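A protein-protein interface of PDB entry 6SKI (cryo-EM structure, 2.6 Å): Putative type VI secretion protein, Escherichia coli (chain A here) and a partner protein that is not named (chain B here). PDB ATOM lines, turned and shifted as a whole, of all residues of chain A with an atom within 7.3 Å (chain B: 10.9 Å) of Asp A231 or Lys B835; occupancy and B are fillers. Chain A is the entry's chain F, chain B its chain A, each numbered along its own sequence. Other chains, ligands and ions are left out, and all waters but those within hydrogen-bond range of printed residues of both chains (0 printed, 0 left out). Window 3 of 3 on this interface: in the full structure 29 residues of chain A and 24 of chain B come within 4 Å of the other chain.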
ATOM      1  N   LYS A   3       3.758 -36.122 -30.612  1.00  0.00           N
ATOM      2  CA  LYS A   3       3.813 -34.670 -30.714  1.00  0.00           C
ATOM      3  C   LYS A   3       4.251 -34.040 -29.396  1.00  0.00           C
ATOM      4  O   LYS A   3       4.708 -32.902 -29.366  1.00  0.00           O
ATOM      5  CB  LYS A   3       2.456 -34.110 -31.143  1.00  0.00           C
ATOM      6  CG  LYS A   3       2.497 -32.659 -31.599  1.00  0.00           C
ATOM      7  CD  LYS A   3       1.122 -32.161 -31.997  1.00  0.00           C
ATOM      8  CE  LYS A   3       0.554 -32.980 -33.142  1.00  0.00           C
ATOM      9  NZ  LYS A   3      -0.629 -33.777 -32.725  1.00  0.00           N
ATOM     10  N   TYR A   4       4.116 -34.788 -28.306  1.00  0.00           N
ATOM     11  CA  TYR A   4       4.494 -34.310 -26.987  1.00  0.00           C
ATOM     12  C   TYR A   4       5.570 -35.214 -26.407  1.00  0.00           C
ATOM     13  O   TYR A   4       5.666 -36.395 -26.751  1.00  0.00           O
ATOM     14  CB  TYR A   4       3.284 -34.245 -26.053  1.00  0.00           C
ATOM     15  CG  TYR A   4       2.140 -33.460 -26.645  1.00  0.00           C
ATOM     16  CD1 TYR A   4       2.214 -32.082 -26.771  1.00  0.00           C
ATOM     17  CD2 TYR A   4       0.998 -34.098 -27.101  1.00  0.00           C
ATOM     18  CE1 TYR A   4       1.179 -31.363 -27.323  1.00  0.00           C
ATOM     19  CE2 TYR A   4      -0.040 -33.386 -27.655  1.00  0.00           C
ATOM     20  CZ  TYR A   4       0.055 -32.019 -27.762  1.00  0.00           C
ATOM     21  OH  TYR A   4      -0.981 -31.308 -28.317  1.00  0.00           O
ATOM     22  N   GLN A   5       6.392 -34.642 -25.534  1.00  0.00           N
ATOM     23  CA  GLN A   5       7.550 -35.338 -24.999  1.00  0.00           C
ATOM     24  C   GLN A   5       7.738 -34.983 -23.536  1.00  0.00           C
ATOM     25  O   GLN A   5       7.550 -33.832 -23.138  1.00  0.00           O
ATOM     26  CB  GLN A   5       8.816 -34.975 -25.775  1.00  0.00           C
ATOM     27  CG  GLN A   5       9.725 -36.141 -26.073  1.00  0.00           C
ATOM     28  CD  GLN A   5      11.032 -35.689 -26.670  1.00  0.00           C
ATOM     29  OE1 GLN A   5      11.675 -34.776 -26.154  1.00  0.00           O
ATOM     30  NE2 GLN A   5      11.430 -36.315 -27.768  1.00  0.00           N
ATOM     31  N   VAL A  35      -3.708 -35.781 -23.937  1.00  0.00           N
ATOM     32  CA  VAL A  35      -5.030 -36.064 -23.390  1.00  0.00           C
ATOM     33  C   VAL A  35      -5.923 -34.844 -23.573  1.00  0.00           C
ATOM     34  O   VAL A  35      -5.517 -33.713 -23.290  1.00  0.00           O
ATOM     35  CB  VAL A  35      -4.950 -36.505 -21.917  1.00  0.00           C
ATOM     36  CG1 VAL A  35      -3.861 -37.545 -21.751  1.00  0.00           C
ATOM     37  CG2 VAL A  35      -4.700 -35.340 -20.985  1.00  0.00           C
ATOM     38  N   CYS A 185       0.692 -35.023 -21.433  1.00  0.00           N
ATOM     39  CA  CYS A 185       0.460 -33.601 -21.591  1.00  0.00           C
ATOM     40  C   CYS A 185      -1.001 -33.384 -21.954  1.00  0.00           C
ATOM     41  O   CYS A 185      -1.581 -34.159 -22.723  1.00  0.00           O
ATOM     42  CB  CYS A 185       1.363 -33.018 -22.676  1.00  0.00           C
ATOM     43  SG  CYS A 185       1.149 -31.256 -22.941  1.00  0.00           S
ATOM     44  N   ILE A 186      -1.598 -32.339 -21.393  1.00  0.00           N
ATOM     45  CA  ILE A 186      -2.967 -31.979 -21.738  1.00  0.00           C
ATOM     46  C   ILE A 186      -2.926 -31.280 -23.090  1.00  0.00           C
ATOM     47  O   ILE A 186      -2.484 -30.135 -23.199  1.00  0.00           O
ATOM     48  CB  ILE A 186      -3.607 -31.098 -20.663  1.00  0.00           C
ATOM     49  CG1 ILE A 186      -3.660 -31.860 -19.341  1.00  0.00           C
ATOM     50  CG2 ILE A 186      -5.000 -30.677 -21.084  1.00  0.00           C
ATOM     51  CD1 ILE A 186      -4.085 -31.027 -18.169  1.00  0.00           C
ATOM     52  N   ALA A 187      -3.390 -31.971 -24.124  1.00  0.00           N
ATOM     53  CA  ALA A 187      -3.299 -31.475 -25.486  1.00  0.00           C
ATOM     54  C   ALA A 187      -4.433 -30.535 -25.845  1.00  0.00           C
ATOM     55  O   ALA A 187      -4.358 -29.859 -26.876  1.00  0.00           O
ATOM     56  CB  ALA A 187      -3.286 -32.644 -26.472  1.00  0.00           C
ATOM     57  N   LYS A 188      -5.478 -30.485 -25.027  1.00  0.00           N
ATOM     58  CA  LYS A 188      -6.619 -29.626 -25.287  1.00  0.00           C
ATOM     59  C   LYS A 188      -7.394 -29.455 -23.994  1.00  0.00           C
ATOM     60  O   LYS A 188      -7.524 -30.400 -23.215  1.00  0.00           O
ATOM     61  CB  LYS A 188      -7.520 -30.217 -26.374  1.00  0.00           C
ATOM     62  CG  LYS A 188      -8.415 -29.211 -27.056  1.00  0.00           C
ATOM     63  CD  LYS A 188      -9.232 -29.878 -28.141  1.00  0.00           C
ATOM     64  CE  LYS A 188     -10.374 -28.992 -28.592  1.00  0.00           C
ATOM     65  NZ  LYS A 188     -10.885 -29.399 -29.928  1.00  0.00           N
ATOM     66  N   ILE A 189      -7.896 -28.250 -23.769  1.00  0.00           N
ATOM     67  CA  ILE A 189      -8.789 -27.958 -22.657  1.00  0.00           C
ATOM     68  C   ILE A 189     -10.150 -27.648 -23.256  1.00  0.00           C
ATOM     69  O   ILE A 189     -10.321 -26.635 -23.946  1.00  0.00           O
ATOM     70  CB  ILE A 189      -8.282 -26.797 -21.795  1.00  0.00           C
ATOM     71  CG1 ILE A 189      -7.006 -27.195 -21.055  1.00  0.00           C
ATOM     72  CG2 ILE A 189      -9.360 -26.350 -20.824  1.00  0.00           C
ATOM     73  CD1 ILE A 189      -7.247 -27.942 -19.773  1.00  0.00           C
ATOM     74  N   LEU A 225      -3.072 -25.940 -13.434  1.00  0.00           N
ATOM     75  CA  LEU A 225      -2.008 -26.825 -13.878  1.00  0.00           C
ATOM     76  C   LEU A 225      -0.668 -26.486 -13.244  1.00  0.00           C
ATOM     77  O   LEU A 225       0.294 -27.235 -13.434  1.00  0.00           O
ATOM     78  CB  LEU A 225      -1.885 -26.775 -15.400  1.00  0.00           C
ATOM     79  CG  LEU A 225      -3.060 -27.397 -16.152  1.00  0.00           C
ATOM     80  CD1 LEU A 225      -2.702 -27.630 -17.605  1.00  0.00           C
ATOM     81  CD2 LEU A 225      -3.488 -28.689 -15.487  1.00  0.00           C
ATOM     82  N   ASP A 228       2.121 -26.086 -15.778  1.00  0.00           N
ATOM     83  CA  ASP A 228       2.316 -27.168 -16.731  1.00  0.00           C
ATOM     84  C   ASP A 228       1.879 -26.745 -18.127  1.00  0.00           C
ATOM     85  O   ASP A 228       0.945 -25.959 -18.301  1.00  0.00           O
ATOM     86  CB  ASP A 228       1.539 -28.409 -16.300  1.00  0.00           C
ATOM     87  CG  ASP A 228       2.115 -29.055 -15.063  1.00  0.00           C
ATOM     88  OD1 ASP A 228       3.114 -28.530 -14.530  1.00  0.00           O
ATOM     89  OD2 ASP A 228       1.571 -30.087 -14.622  1.00  0.00           O
ATOM     90  N   PHE A 229       2.571 -27.278 -19.127  1.00  0.00           N
ATOM     91  CA  PHE A 229       2.235 -26.976 -20.508  1.00  0.00           C
ATOM     92  C   PHE A 229       0.935 -27.661 -20.904  1.00  0.00           C
ATOM     93  O   PHE A 229       0.742 -28.854 -20.652  1.00  0.00           O
ATOM     94  CB  PHE A 229       3.362 -27.427 -21.434  1.00  0.00           C
ATOM     95  CG  PHE A 229       3.012 -27.357 -22.887  1.00  0.00           C
ATOM     96  CD1 PHE A 229       2.922 -28.506 -23.643  1.00  0.00           C
ATOM     97  CD2 PHE A 229       2.788 -26.141 -23.500  1.00  0.00           C
ATOM     98  CE1 PHE A 229       2.598 -28.447 -24.975  1.00  0.00           C
ATOM     99  CE2 PHE A 229       2.467 -26.077 -24.836  1.00  0.00           C
ATOM    100  CZ  PHE A 229       2.371 -27.232 -25.574  1.00  0.00           C
ATOM    101  N   TYR A 230       0.037 -26.901 -21.522  1.00  0.00           N
ATOM    102  CA  TYR A 230      -1.153 -27.469 -22.139  1.00  0.00           C
ATOM    103  C   TYR A 230      -1.280 -26.908 -23.544  1.00  0.00           C
ATOM    104  O   TYR A 230      -1.121 -25.701 -23.751  1.00  0.00           O
ATOM    105  CB  TYR A 230      -2.421 -27.185 -21.325  1.00  0.00           C
ATOM    106  CG  TYR A 230      -2.727 -25.728 -21.064  1.00  0.00           C
ATOM    107  CD1 TYR A 230      -2.213 -25.079 -19.956  1.00  0.00           C
ATOM    108  CD2 TYR A 230      -3.568 -25.017 -21.905  1.00  0.00           C
ATOM    109  CE1 TYR A 230      -2.504 -23.760 -19.708  1.00  0.00           C
ATOM    110  CE2 TYR A 230      -3.864 -23.700 -21.664  1.00  0.00           C
ATOM    111  CZ  TYR A 230      -3.331 -23.076 -20.564  1.00  0.00           C
ATOM    112  OH  TYR A 230      -3.625 -21.756 -20.323  1.00  0.00           O
ATOM    113  N   ASP A 231      -1.552 -27.783 -24.503  1.00  0.00           N
ATOM    114  CA  ASP A 231      -1.675 -27.374 -25.890  1.00  0.00           C
ATOM    115  C   ASP A 231      -3.076 -26.826 -26.149  1.00  0.00           C
ATOM    116  O   ASP A 231      -3.935 -26.793 -25.265  1.00  0.00           O
ATOM    117  CB  ASP A 231      -1.353 -28.547 -26.810  1.00  0.00           C
ATOM    118  CG  ASP A 231      -0.772 -28.107 -28.131  1.00  0.00           C
ATOM    119  OD1 ASP A 231      -0.194 -27.005 -28.187  1.00  0.00           O
ATOM    120  OD2 ASP A 231      -0.888 -28.865 -29.115  1.00  0.00           O
ATOM    121  N   GLY A 232      -3.312 -26.379 -27.375  1.00  0.00           N
ATOM    122  CA  GLY A 232      -4.607 -25.843 -27.730  1.00  0.00           C
ATOM    123  C   GLY A 232      -4.726 -24.372 -27.406  1.00  0.00           C
ATOM    124  O   GLY A 232      -3.771 -23.700 -27.005  1.00  0.00           O
ATOM    125  N   LYS A 233      -5.935 -23.860 -27.599  1.00  0.00           N
ATOM    126  CA  LYS A 233      -6.223 -22.476 -27.259  1.00  0.00           C
ATOM    127  C   LYS A 233      -5.948 -22.245 -25.777  1.00  0.00           C
ATOM    128  O   LYS A 233      -6.425 -23.017 -24.936  1.00  0.00           O
ATOM    129  CB  LYS A 233      -7.674 -22.138 -27.588  1.00  0.00           C
ATOM    130  CG  LYS A 233      -7.990 -22.182 -29.070  1.00  0.00           C
ATOM    131  CD  LYS A 233      -9.484 -22.205 -29.310  1.00  0.00           C
ATOM    132  CE  LYS A 233      -9.802 -22.377 -30.783  1.00  0.00           C
ATOM    133  NZ  LYS A 233      -9.255 -23.649 -31.327  1.00  0.00           N
ATOM    134  N   PRO A 234      -5.192 -21.204 -25.418  1.00  0.00           N
ATOM    135  CA  PRO A 234      -4.799 -21.033 -24.010  1.00  0.00           C
ATOM    136  C   PRO A 234      -5.966 -20.846 -23.061  1.00  0.00           C
ATOM    137  O   PRO A 234      -5.835 -21.156 -21.872  1.00  0.00           O
ATOM    138  CB  PRO A 234      -3.903 -19.790 -24.065  1.00  0.00           C
ATOM    139  CG  PRO A 234      -4.422 -19.043 -25.249  1.00  0.00           C
ATOM    140  CD  PRO A 234      -4.643 -20.128 -26.255  1.00  0.00           C
ATOM    141  N   GLY A 236      -8.984 -22.285 -23.782  1.00  0.00           N
ATOM    142  CA  GLY A 236      -9.818 -23.453 -23.947  1.00  0.00           C
ATOM    143  C   GLY A 236     -10.803 -23.315 -25.085  1.00  0.00           C
ATOM    144  O   GLY A 236     -10.808 -22.350 -25.852  1.00  0.00           O
ATOM    145  N   GLN B 791      18.463 -29.720 -23.147  1.00  0.00           N
ATOM    146  CA  GLN B 791      17.103 -29.552 -23.648  1.00  0.00           C
ATOM    147  C   GLN B 791      16.670 -28.100 -23.499  1.00  0.00           C
ATOM    148  O   GLN B 791      16.606 -27.599 -22.367  1.00  0.00           O
ATOM    149  CB  GLN B 791      16.151 -30.470 -22.903  1.00  0.00           C
ATOM    150  CG  GLN B 791      16.654 -31.895 -22.822  1.00  0.00           C
ATOM    151  CD  GLN B 791      16.581 -32.605 -24.154  1.00  0.00           C
ATOM    152  OE1 GLN B 791      15.850 -32.193 -25.052  1.00  0.00           O
ATOM    153  NE2 GLN B 791      17.347 -33.677 -24.295  1.00  0.00           N
ATOM    154  N   PRO B 792      16.330 -27.406 -24.585  1.00  0.00           N
ATOM    155  CA  PRO B 792      16.250 -25.939 -24.540  1.00  0.00           C
ATOM    156  C   PRO B 792      15.069 -25.340 -23.786  1.00  0.00           C
ATOM    157  O   PRO B 792      15.279 -24.461 -22.948  1.00  0.00           O
ATOM    158  CB  PRO B 792      16.201 -25.569 -26.027  1.00  0.00           C
ATOM    159  CG  PRO B 792      15.474 -26.708 -26.653  1.00  0.00           C
ATOM    160  CD  PRO B 792      15.904 -27.943 -25.889  1.00  0.00           C
ATOM    161  N   SER B 793      13.837 -25.768 -24.044  1.00  0.00           N
ATOM    162  CA  SER B 793      12.683 -25.026 -23.542  1.00  0.00           C
ATOM    163  C   SER B 793      11.752 -25.919 -22.737  1.00  0.00           C
ATOM    164  O   SER B 793      10.525 -25.817 -22.833  1.00  0.00           O
ATOM    165  CB  SER B 793      11.927 -24.359 -24.688  1.00  0.00           C
ATOM    166  N   THR B 794      12.320 -26.803 -21.929  1.00  0.00           N
ATOM    167  CA  THR B 794      11.509 -27.648 -21.068  1.00  0.00           C
ATOM    168  C   THR B 794      10.929 -26.835 -19.913  1.00  0.00           C
ATOM    169  O   THR B 794      11.635 -26.016 -19.315  1.00  0.00           O
ATOM    170  CB  THR B 794      12.347 -28.802 -20.522  1.00  0.00           C
ATOM    171  OG1 THR B 794      12.941 -29.517 -21.612  1.00  0.00           O
ATOM    172  CG2 THR B 794      11.485 -29.752 -19.710  1.00  0.00           C
ATOM    173  N   PRO B 795       9.655 -27.020 -19.583  1.00  0.00           N
ATOM    174  CA  PRO B 795       9.126 -26.438 -18.346  1.00  0.00           C
ATOM    175  C   PRO B 795       9.686 -27.149 -17.126  1.00  0.00           C
ATOM    176  O   PRO B 795      10.054 -28.324 -17.177  1.00  0.00           O
ATOM    177  CB  PRO B 795       7.614 -26.659 -18.470  1.00  0.00           C
ATOM    178  CG  PRO B 795       7.384 -26.829 -19.935  1.00  0.00           C
ATOM    179  CD  PRO B 795       8.581 -27.581 -20.415  1.00  0.00           C
ATOM    180  N   ILE B 809      10.855 -22.006 -17.253  1.00  0.00           N
ATOM    181  CA  ILE B 809      11.217 -22.795 -18.424  1.00  0.00           C
ATOM    182  C   ILE B 809      12.722 -22.684 -18.625  1.00  0.00           C
ATOM    183  O   ILE B 809      13.286 -21.588 -18.543  1.00  0.00           O
ATOM    184  CB  ILE B 809      10.457 -22.323 -19.681  1.00  0.00           C
ATOM    185  CG1 ILE B 809       8.959 -22.586 -19.527  1.00  0.00           C
ATOM    186  CG2 ILE B 809      10.988 -23.011 -20.924  1.00  0.00           C
ATOM    187  CD1 ILE B 809       8.095 -21.387 -19.836  1.00  0.00           C
ATOM    188  N   GLY B 832       8.472 -30.517 -16.872  1.00  0.00           N
ATOM    189  CA  GLY B 832       7.217 -30.689 -17.575  1.00  0.00           C
ATOM    190  C   GLY B 832       7.386 -31.354 -18.921  1.00  0.00           C
ATOM    191  O   GLY B 832       8.298 -32.157 -19.136  1.00  0.00           O
ATOM    192  N   LYS B 833       6.494 -31.012 -19.845  1.00  0.00           N
ATOM    193  CA  LYS B 833       6.460 -31.625 -21.162  1.00  0.00           C
ATOM    194  C   LYS B 833       6.672 -30.566 -22.234  1.00  0.00           C
ATOM    195  O   LYS B 833       6.444 -29.375 -22.016  1.00  0.00           O
ATOM    196  CB  LYS B 833       5.134 -32.354 -21.401  1.00  0.00           C
ATOM    197  CG  LYS B 833       4.573 -33.030 -20.167  1.00  0.00           C
ATOM    198  CD  LYS B 833       4.905 -34.506 -20.131  1.00  0.00           C
ATOM    199  CE  LYS B 833       4.913 -35.021 -18.706  1.00  0.00           C
ATOM    200  NZ  LYS B 833       5.764 -36.230 -18.563  1.00  0.00           N
ATOM    201  N   VAL B 834       7.110 -31.020 -23.409  1.00  0.00           N
ATOM    202  CA  VAL B 834       7.418 -30.139 -24.527  1.00  0.00           C
ATOM    203  C   VAL B 834       6.738 -30.673 -25.777  1.00  0.00           C
ATOM    204  O   VAL B 834       6.414 -31.856 -25.884  1.00  0.00           O
ATOM    205  CB  VAL B 834       8.937 -30.001 -24.776  1.00  0.00           C
ATOM    206  CG1 VAL B 834       9.633 -29.461 -23.550  1.00  0.00           C
ATOM    207  CG2 VAL B 834       9.532 -31.333 -25.190  1.00  0.00           C
ATOM    208  N   LYS B 835       6.524 -29.774 -26.730  1.00  0.00           N
ATOM    209  CA  LYS B 835       5.889 -30.126 -27.989  1.00  0.00           C
ATOM    210  C   LYS B 835       6.932 -30.487 -29.042  1.00  0.00           C
ATOM    211  O   LYS B 835       7.228 -31.661 -29.264  1.00  0.00           O
ATOM    212  CB  LYS B 835       5.019 -28.969 -28.479  1.00  0.00           C
ATOM    213  CG  LYS B 835       3.781 -29.396 -29.234  1.00  0.00           C
ATOM    214  CD  LYS B 835       2.954 -28.192 -29.629  1.00  0.00           C
ATOM    215  CE  LYS B 835       2.082 -28.496 -30.832  1.00  0.00           C
ATOM    216  NZ  LYS B 835       1.557 -27.255 -31.457  1.00  0.00           N
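The backbone carbonyl oxygen of Val B834 is in hydrogen-bond range of the backbone NH of Gln A5, 2.8 Å away.
The side-chain carboxylate (OD1) of Asp A231 is in salt-bridge range of the side-chain amino group (NZ) of Lys B835, at 3.7 Å.
The backbone carbonyl oxygen (O) of Lys B835 sits close to the backbone carbonyl oxygen (O) of Lys A3 (2.8 Å).
N of Asp A231 lies within hydrogen-bond range of O of Ile A186 (2.8 Å).
SG of Cys A185 lies within hydrogen-bond range of O of Phe A229 (3.3 Å).
OH of Tyr A4 is in hydrogen-bond range of OD2 of Asp A231, 2.6 Å away.
Tyr A4 touches Val B834 (CA to O, 3.3 Å).
Tyr A4 touches Lys B835 (CE1 to CG, 3.8 Å).
Lys B833 touches Gln A5 (CA to O, 3.2 Å).
O of Lys B833 touches CB of Phe A229 (3.7 Å).
Printed residues of chain B within 4 Å of Asp A231: Lys B835 (3.5 Å).
Of chain B, only Val B834 (3.3 Å) and Lys B835 (3.8 Å) come within 4 Å of Tyr A4.
Of chain B, only Lys B833 and Val B834 come within 4 Å of Gln A5.
Of chain B, only Lys B833 (3.7 Å) comes within 4 Å of Phe A229.
No residue of chain B comes within 4 Å of Gly A232.
Of the printed residues of chain B, Lys A3 touches Lys B835 (2.8 Å).
Printed residues of chain A within 4 Å of Val B834: Tyr A4 (3.3 Å) and Gln A5 (2.8 Å).
Of the printed residues of chain A, Lys B833 touches Gln A5 and Phe A229.
Thr B794 touches none of the printed residues of chain A.
The nearest residue of chain B that does not touch Asp A231 is Val B834 (8.2 Å).
The nearest printed residue of chain A that does not touch Val B834 is Lys A3 (4.02 Å).
Printed residues of chain B that touch a printed residue of chain A: Lys B833, Val B834 and Lys B835.
Hydrophobic or aromatic side chains of chain A that line the printed part of chain B: Tyr A4 and Phe A229.
Among the printed residues, 7 pairs touch across the chains.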
